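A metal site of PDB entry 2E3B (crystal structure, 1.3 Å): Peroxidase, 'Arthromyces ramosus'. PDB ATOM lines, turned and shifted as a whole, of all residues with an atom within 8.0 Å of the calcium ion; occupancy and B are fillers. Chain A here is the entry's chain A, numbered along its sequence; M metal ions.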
ATOM      1  N   PRO A 130      11.228  -2.944  -6.685  1.00  0.00           N
ATOM      2  CA  PRO A 130      11.556  -2.000  -5.642  1.00  0.00           C
ATOM      3  C   PRO A 130      13.016  -1.649  -5.586  1.00  0.00           C
ATOM      4  O   PRO A 130      13.865  -2.493  -5.685  1.00  0.00           O
ATOM      5  CB  PRO A 130      11.181  -2.808  -4.401  1.00  0.00           C
ATOM      6  CG  PRO A 130       9.954  -3.530  -4.849  1.00  0.00           C
ATOM      7  CD  PRO A 130      10.327  -4.023  -6.246  1.00  0.00           C
ATOM      8  N   ALA A 182      24.873  -5.151 -11.352  1.00  0.00           N
ATOM      9  CA  ALA A 182      23.826  -4.895 -10.365  1.00  0.00           C
ATOM     10  C   ALA A 182      22.551  -5.622 -10.797  1.00  0.00           C
ATOM     11  O   ALA A 182      21.754  -5.931  -9.940  1.00  0.00           O
ATOM     12  CB  ALA A 182      23.553  -3.421 -10.205  1.00  0.00           C
ATOM     13  N   ALA A 183      22.350  -5.928 -12.063  1.00  0.00           N
ATOM     14  CA  ALA A 183      21.189  -6.678 -12.481  1.00  0.00           C
ATOM     15  C   ALA A 183      21.152  -8.051 -11.816  1.00  0.00           C
ATOM     16  O   ALA A 183      20.068  -8.612 -11.668  1.00  0.00           O
ATOM     17  CB  ALA A 183      21.164  -6.862 -13.978  1.00  0.00           C
ATOM     18  N   HIS A 184      22.259  -8.596 -11.371  1.00  0.00           N
ATOM     19  CA  HIS A 184      22.223  -9.854 -10.663  1.00  0.00           C
ATOM     20  C   HIS A 184      21.639  -9.703  -9.275  1.00  0.00           C
ATOM     21  O   HIS A 184      21.456 -10.710  -8.597  1.00  0.00           O
ATOM     22  CB  HIS A 184      23.597 -10.531 -10.627  1.00  0.00           C
ATOM     23  CG  HIS A 184      23.932 -11.217 -11.909  1.00  0.00           C
ATOM     24  ND1 HIS A 184      24.992 -12.083 -12.034  1.00  0.00           N
ATOM     25  CD2 HIS A 184      23.371 -11.149 -13.141  1.00  0.00           C
ATOM     26  CE1 HIS A 184      25.041 -12.514 -13.277  1.00  0.00           C
ATOM     27  NE2 HIS A 184      24.064 -11.983 -13.996  1.00  0.00           N
ATOM     28  N   SER A 185      21.306  -8.475  -8.886  1.00  0.00           N
ATOM     29  CA  SER A 185      20.430  -8.265  -7.723  1.00  0.00           C
ATOM     30  C   SER A 185      18.995  -8.668  -7.969  1.00  0.00           C
ATOM     31  O   SER A 185      18.225  -8.733  -7.020  1.00  0.00           O
ATOM     32  CB  SER A 185      20.496  -6.794  -7.324  1.00  0.00           C
ATOM     33  OG  SER A 185      19.884  -6.608  -6.061  1.00  0.00           O
ATOM     34  N   LEU A 186      18.612  -8.923  -9.200  1.00  0.00           N
ATOM     35  CA  LEU A 186      17.255  -9.304  -9.537  1.00  0.00           C
ATOM     36  C   LEU A 186      17.360 -10.556 -10.357  1.00  0.00           C
ATOM     37  O   LEU A 186      17.033 -10.576 -11.533  1.00  0.00           O
ATOM     38  CB  LEU A 186      16.613  -8.234 -10.395  1.00  0.00           C
ATOM     39  CG  LEU A 186      16.389  -6.900  -9.702  1.00  0.00           C
ATOM     40  CD1 LEU A 186      15.901  -5.914 -10.768  1.00  0.00           C
ATOM     41  CD2 LEU A 186      15.398  -6.994  -8.561  1.00  0.00           C
ATOM     42  N   ALA A 187      17.836 -11.642  -9.745  1.00  0.00           N
ATOM     43  CA  ALA A 187      18.331 -12.705 -10.572  1.00  0.00           C
ATOM     44  C   ALA A 187      18.246 -14.083  -9.912  1.00  0.00           C
ATOM     45  O   ALA A 187      18.337 -14.278  -8.709  1.00  0.00           O
ATOM     46  CB  ALA A 187      19.812 -12.470 -10.910  1.00  0.00           C
ATOM     47  N   PRO A 200      17.908 -18.040  -6.418  1.00  0.00           N
ATOM     48  CA  PRO A 200      18.371 -16.657  -6.600  1.00  0.00           C
ATOM     49  C   PRO A 200      19.866 -16.491  -6.422  1.00  0.00           C
ATOM     50  O   PRO A 200      20.582 -17.251  -5.786  1.00  0.00           O
ATOM     51  CB  PRO A 200      17.650 -15.916  -5.472  1.00  0.00           C
ATOM     52  CG  PRO A 200      16.476 -16.770  -5.124  1.00  0.00           C
ATOM     53  CD  PRO A 200      17.052 -18.147  -5.211  1.00  0.00           C
ATOM     54  N   LEU A 201      20.357 -15.428  -7.067  1.00  0.00           N
ATOM     55  CA  LEU A 201      21.741 -14.992  -6.926  1.00  0.00           C
ATOM     56  C   LEU A 201      21.939 -14.094  -5.732  1.00  0.00           C
ATOM     57  O   LEU A 201      23.074 -13.923  -5.316  1.00  0.00           O
ATOM     58  CB  LEU A 201      22.229 -14.339  -8.191  1.00  0.00           C
ATOM     59  CG  LEU A 201      21.997 -15.053  -9.506  1.00  0.00           C
ATOM     60  CD1 LEU A 201      22.699 -14.315 -10.654  1.00  0.00           C
ATOM     61  CD2 LEU A 201      22.522 -16.492  -9.435  1.00  0.00           C
ATOM     62  N   ASP A 202      20.891 -13.514  -5.218  1.00  0.00           N
ATOM     63  CA  ASP A 202      20.980 -12.777  -3.973  1.00  0.00           C
ATOM     64  C   ASP A 202      19.688 -13.050  -3.201  1.00  0.00           C
ATOM     65  O   ASP A 202      18.744 -13.604  -3.723  1.00  0.00           O
ATOM     66  CB  ASP A 202      21.295 -11.320  -4.114  1.00  0.00           C
ATOM     67  CG  ASP A 202      20.200 -10.315  -4.380  1.00  0.00           C
ATOM     68  OD1 ASP A 202      19.014 -10.640  -4.480  1.00  0.00           O
ATOM     69  OD2 ASP A 202      20.571  -9.126  -4.484  1.00  0.00           O
ATOM     70  N   SER A 203      19.676 -12.676  -1.937  1.00  0.00           N
ATOM     71  CA  SER A 203      18.573 -13.008  -1.056  1.00  0.00           C
ATOM     72  C   SER A 203      17.319 -12.190  -1.351  1.00  0.00           C
ATOM     73  O   SER A 203      16.287 -12.501  -0.777  1.00  0.00           O
ATOM     74  CB  SER A 203      18.943 -12.820   0.406  1.00  0.00           C
ATOM     75  OG  SER A 203      19.278 -11.469   0.674  1.00  0.00           O
ATOM     76  N   THR A 204      17.420 -11.219  -2.238  1.00  0.00           N
ATOM     77  CA  THR A 204      16.292 -10.366  -2.548  1.00  0.00           C
ATOM     78  C   THR A 204      16.123 -10.235  -4.040  1.00  0.00           C
ATOM     79  O   THR A 204      16.306  -9.169  -4.617  1.00  0.00           O
ATOM     80  CB  THR A 204      16.515  -8.980  -1.913  1.00  0.00           C
ATOM     81  OG1 THR A 204      17.764  -8.448  -2.378  1.00  0.00           O
ATOM     82  CG2 THR A 204      16.600  -9.088  -0.402  1.00  0.00           C
ATOM     83  N   PRO A 205      15.754 -11.310  -4.728  1.00  0.00           N
ATOM     84  CA  PRO A 205      15.702 -11.235  -6.175  1.00  0.00           C
ATOM     85  C   PRO A 205      14.549 -10.389  -6.671  1.00  0.00           C
ATOM     86  O   PRO A 205      14.491 -10.236  -7.903  1.00  0.00           O
ATOM     87  CB  PRO A 205      15.534 -12.713  -6.615  1.00  0.00           C
ATOM     88  CG  PRO A 205      14.817 -13.336  -5.440  1.00  0.00           C
ATOM     89  CD  PRO A 205      15.435 -12.646  -4.267  1.00  0.00           C
ATOM     90  N   GLN A 206      13.722  -9.876  -5.791  1.00  0.00           N
ATOM     91  CA  GLN A 206      12.710  -8.924  -6.202  1.00  0.00           C
ATOM     92  C   GLN A 206      12.988  -7.551  -5.651  1.00  0.00           C
ATOM     93  O   GLN A 206      12.076  -6.724  -5.681  1.00  0.00           O
ATOM     94  CB  GLN A 206      11.346  -9.377  -5.707  1.00  0.00           C
ATOM     95  CG  GLN A 206      10.922 -10.697  -6.373  1.00  0.00           C
ATOM     96  CD  GLN A 206       9.477 -10.999  -5.960  1.00  0.00           C
ATOM     97  OE1 GLN A 206       9.285 -11.509  -4.863  1.00  0.00           O
ATOM     98  NE2 GLN A 206       8.595 -10.682  -6.867  1.00  0.00           N
ATOM     99  N   VAL A 207      14.197  -7.275  -5.180  1.00  0.00           N
ATOM    100  CA  VAL A 207      14.542  -5.935  -4.760  1.00  0.00           C
ATOM    101  C   VAL A 207      15.876  -5.570  -5.389  1.00  0.00           C
ATOM    102  O   VAL A 207      16.830  -6.330  -5.283  1.00  0.00           O
ATOM    103  CB  VAL A 207      14.586  -5.771  -3.232  1.00  0.00           C
ATOM    104  CG1 VAL A 207      14.968  -4.381  -2.820  1.00  0.00           C
ATOM    105  CG2 VAL A 207      13.266  -6.183  -2.602  1.00  0.00           C
ATOM    106  N   PHE A 208      15.884  -4.446  -6.057  1.00  0.00           N
ATOM    107  CA  PHE A 208      17.084  -3.937  -6.692  1.00  0.00           C
ATOM    108  C   PHE A 208      17.892  -3.223  -5.632  1.00  0.00           C
ATOM    109  O   PHE A 208      17.644  -2.060  -5.325  1.00  0.00           O
ATOM    110  CB  PHE A 208      16.719  -3.047  -7.856  1.00  0.00           C
ATOM    111  CG  PHE A 208      17.991  -2.652  -8.598  1.00  0.00           C
ATOM    112  CD1 PHE A 208      18.646  -3.561  -9.408  1.00  0.00           C
ATOM    113  CD2 PHE A 208      18.492  -1.390  -8.475  1.00  0.00           C
ATOM    114  CE1 PHE A 208      19.793  -3.214 -10.095  1.00  0.00           C
ATOM    115  CE2 PHE A 208      19.655  -1.009  -9.110  1.00  0.00           C
ATOM    116  CZ  PHE A 208      20.295  -1.917  -9.937  1.00  0.00           C
ATOM    117  N   ASP A 209      18.797  -3.965  -5.043  1.00  0.00           N
ATOM    118  CA  ASP A 209      19.559  -3.558  -3.861  1.00  0.00           C
ATOM    119  C   ASP A 209      20.974  -4.108  -3.942  1.00  0.00           C
ATOM    120  O   ASP A 209      21.379  -4.793  -4.876  1.00  0.00           O
ATOM    121  CB  ASP A 209      18.870  -3.999  -2.585  1.00  0.00           C
ATOM    122  CG  ASP A 209      18.640  -5.487  -2.513  1.00  0.00           C
ATOM    123  OD1 ASP A 209      19.239  -6.204  -3.331  1.00  0.00           O
ATOM    124  OD2 ASP A 209      17.884  -5.925  -1.653  1.00  0.00           O
ATOM    125  N   THR A 210      21.751  -3.798  -2.895  1.00  0.00           N
ATOM    126  CA  THR A 210      23.134  -4.179  -2.923  1.00  0.00           C
ATOM    127  C   THR A 210      23.384  -5.586  -2.432  1.00  0.00           C
ATOM    128  O   THR A 210      24.532  -5.983  -2.325  1.00  0.00           O
ATOM    129  CB  THR A 210      23.974  -3.258  -2.049  1.00  0.00           C
ATOM    130  OG1 THR A 210      23.509  -3.413  -0.709  1.00  0.00           O
ATOM    131  CG2 THR A 210      23.838  -1.828  -2.509  1.00  0.00           C
ATOM    132  N   GLN A 211      22.341  -6.365  -2.109  1.00  0.00           N
ATOM    133  CA  GLN A 211      22.566  -7.652  -1.506  1.00  0.00           C
ATOM    134  C   GLN A 211      23.443  -8.536  -2.374  1.00  0.00           C
ATOM    135  O   GLN A 211      24.256  -9.269  -1.858  1.00  0.00           O
ATOM    136  CB  GLN A 211      21.229  -8.352  -1.251  1.00  0.00           C
ATOM    137  CG  GLN A 211      20.430  -7.781  -0.110  1.00  0.00           C
ATOM    138  CD  GLN A 211      21.199  -7.546   1.163  1.00  0.00           C
ATOM    139  OE1 GLN A 211      21.138  -6.454   1.722  1.00  0.00           O
ATOM    140  NE2 GLN A 211      21.906  -8.545   1.656  1.00  0.00           N
ATOM    141  N   PHE A 212      23.275  -8.465  -3.695  1.00  0.00           N
ATOM    142  CA  PHE A 212      24.115  -9.287  -4.548  1.00  0.00           C
ATOM    143  C   PHE A 212      25.588  -9.056  -4.302  1.00  0.00           C
ATOM    144  O   PHE A 212      26.387  -9.999  -4.270  1.00  0.00           O
ATOM    145  CB  PHE A 212      23.765  -8.965  -5.998  1.00  0.00           C
ATOM    146  CG  PHE A 212      24.759  -9.520  -7.006  1.00  0.00           C
ATOM    147  CD1 PHE A 212      24.829 -10.860  -7.297  1.00  0.00           C
ATOM    148  CD2 PHE A 212      25.627  -8.674  -7.645  1.00  0.00           C
ATOM    149  CE1 PHE A 212      25.743 -11.352  -8.193  1.00  0.00           C
ATOM    150  CE2 PHE A 212      26.528  -9.153  -8.553  1.00  0.00           C
ATOM    151  CZ  PHE A 212      26.610 -10.490  -8.836  1.00  0.00           C
ATOM    152  N   TYR A 213      25.996  -7.820  -4.140  1.00  0.00           N
ATOM    153  CA  TYR A 213      27.409  -7.512  -3.990  1.00  0.00           C
ATOM    154  C   TYR A 213      27.895  -7.978  -2.637  1.00  0.00           C
ATOM    155  O   TYR A 213      29.010  -8.477  -2.544  1.00  0.00           O
ATOM    156  CB  TYR A 213      27.622  -6.045  -4.154  1.00  0.00           C
ATOM    157  CG  TYR A 213      27.382  -5.552  -5.563  1.00  0.00           C
ATOM    158  CD1 TYR A 213      28.299  -5.764  -6.571  1.00  0.00           C
ATOM    159  CD2 TYR A 213      26.216  -4.871  -5.853  1.00  0.00           C
ATOM    160  CE1 TYR A 213      28.022  -5.320  -7.846  1.00  0.00           C
ATOM    161  CE2 TYR A 213      25.952  -4.398  -7.133  1.00  0.00           C
ATOM    162  CZ  TYR A 213      26.876  -4.629  -8.106  1.00  0.00           C
ATOM    163  OH  TYR A 213      26.619  -4.129  -9.356  1.00  0.00           O
ATOM    164  N   GLU A 215      26.524 -10.489  -0.844  1.00  0.00           N
ATOM    165  CA  GLU A 215      26.473 -11.923  -0.608  1.00  0.00           C
ATOM    166  C   GLU A 215      27.446 -12.718  -1.458  1.00  0.00           C
ATOM    167  O   GLU A 215      27.861 -13.799  -1.048  1.00  0.00           O
ATOM    168  CB  GLU A 215      25.025 -12.356  -0.847  1.00  0.00           C
ATOM    169  CG  GLU A 215      24.114 -11.799   0.231  1.00  0.00           C
ATOM    170  CD  GLU A 215      22.635 -11.952  -0.074  1.00  0.00           C
ATOM    171  OE1 GLU A 215      22.225 -12.788  -0.884  1.00  0.00           O
ATOM    172  OE2 GLU A 215      21.891 -11.190   0.557  1.00  0.00           O
ATOM    173  N   ASN A 266      22.549   1.608  -1.911  1.00  0.00           N
ATOM    174  CA  ASN A 266      21.625   1.329  -3.001  1.00  0.00           C
ATOM    175  C   ASN A 266      21.562   2.522  -3.956  1.00  0.00           C
ATOM    176  O   ASN A 266      21.364   2.378  -5.140  1.00  0.00           O
ATOM    177  CB  ASN A 266      20.219   1.059  -2.444  1.00  0.00           C
ATOM    178  CG  ASN A 266      20.092  -0.242  -1.693  1.00  0.00           C
ATOM    179  OD1 ASN A 266      20.661  -1.222  -2.096  1.00  0.00           O
ATOM    180  ND2 ASN A 266      19.300  -0.254  -0.636  1.00  0.00           N
ATOM    181  N   MET A 269      24.584   2.625  -6.164  1.00  0.00           N
ATOM    182  CA  MET A 269      24.496   1.485  -7.070  1.00  0.00           C
ATOM    183  C   MET A 269      23.517   1.771  -8.189  1.00  0.00           C
ATOM    184  O   MET A 269      23.800   1.506  -9.350  1.00  0.00           O
ATOM    185  CB  MET A 269      24.043   0.250  -6.299  1.00  0.00           C
ATOM    186  CG  MET A 269      23.860  -0.959  -7.169  1.00  0.00           C
ATOM    187  SD  MET A 269      23.070  -2.334  -6.361  1.00  0.00           S
ATOM    188  CE  MET A 269      21.442  -1.623  -6.146  1.00  0.00           C
ATOM    189  N   ASN A 303      12.661   1.259  -2.162  1.00  0.00           N
ATOM    190  CA  ASN A 303      13.056   0.179  -1.253  1.00  0.00           C
ATOM    191  C   ASN A 303      13.512   0.764   0.061  1.00  0.00           C
ATOM    192  O   ASN A 303      14.489   1.511   0.003  1.00  0.00           O
ATOM    193  CB  ASN A 303      14.231  -0.581  -1.863  1.00  0.00           C
ATOM    194  CG  ASN A 303      14.848  -1.544  -0.875  1.00  0.00           C
ATOM    195  OD1 ASN A 303      14.113  -2.073  -0.046  1.00  0.00           O
ATOM    196  ND2 ASN A 303      16.172  -1.747  -0.937  1.00  0.00           N
HETATM  197 CA    CA M   1      18.414  -8.048  -4.728  1.00  0.00          CA
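The side-chain carboxylate (OD1) of Asp 209 lies close to the backbone NH (N) of Gln 211 (3.3 Å). The backbone NH of Phe 212 sits close to the side-chain carboxylate of Asp 202 (2.9 Å).
The calcium ion is bound by the backbone carbonyl oxygen (O) of Thr 204 (2.4 Å), the backbone carbonyl oxygen (O) of Ser 185 (2.4 Å), the backbone carbonyl oxygen (O) of Val 207 (2.4 Å), the side-chain carboxylate (OD2) of Asp 202 (2.4 Å), the side-chain hydroxyl (OG) of Ser 185 (2.5 Å), the side-chain carboxylate (OD1) of Asp 209 (2.5 Å), the side-chain hydroxyl (OG1) of Thr 204 (2.5 Å) and the side-chain carboxylate (OD1) of Asp 202 (2.7 Å).
Of the 25 residues printed, 5 come within 4 Å of the calcium ion. Along chain A the residues within 4 Å of the calcium ion span positions 185 to 209.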
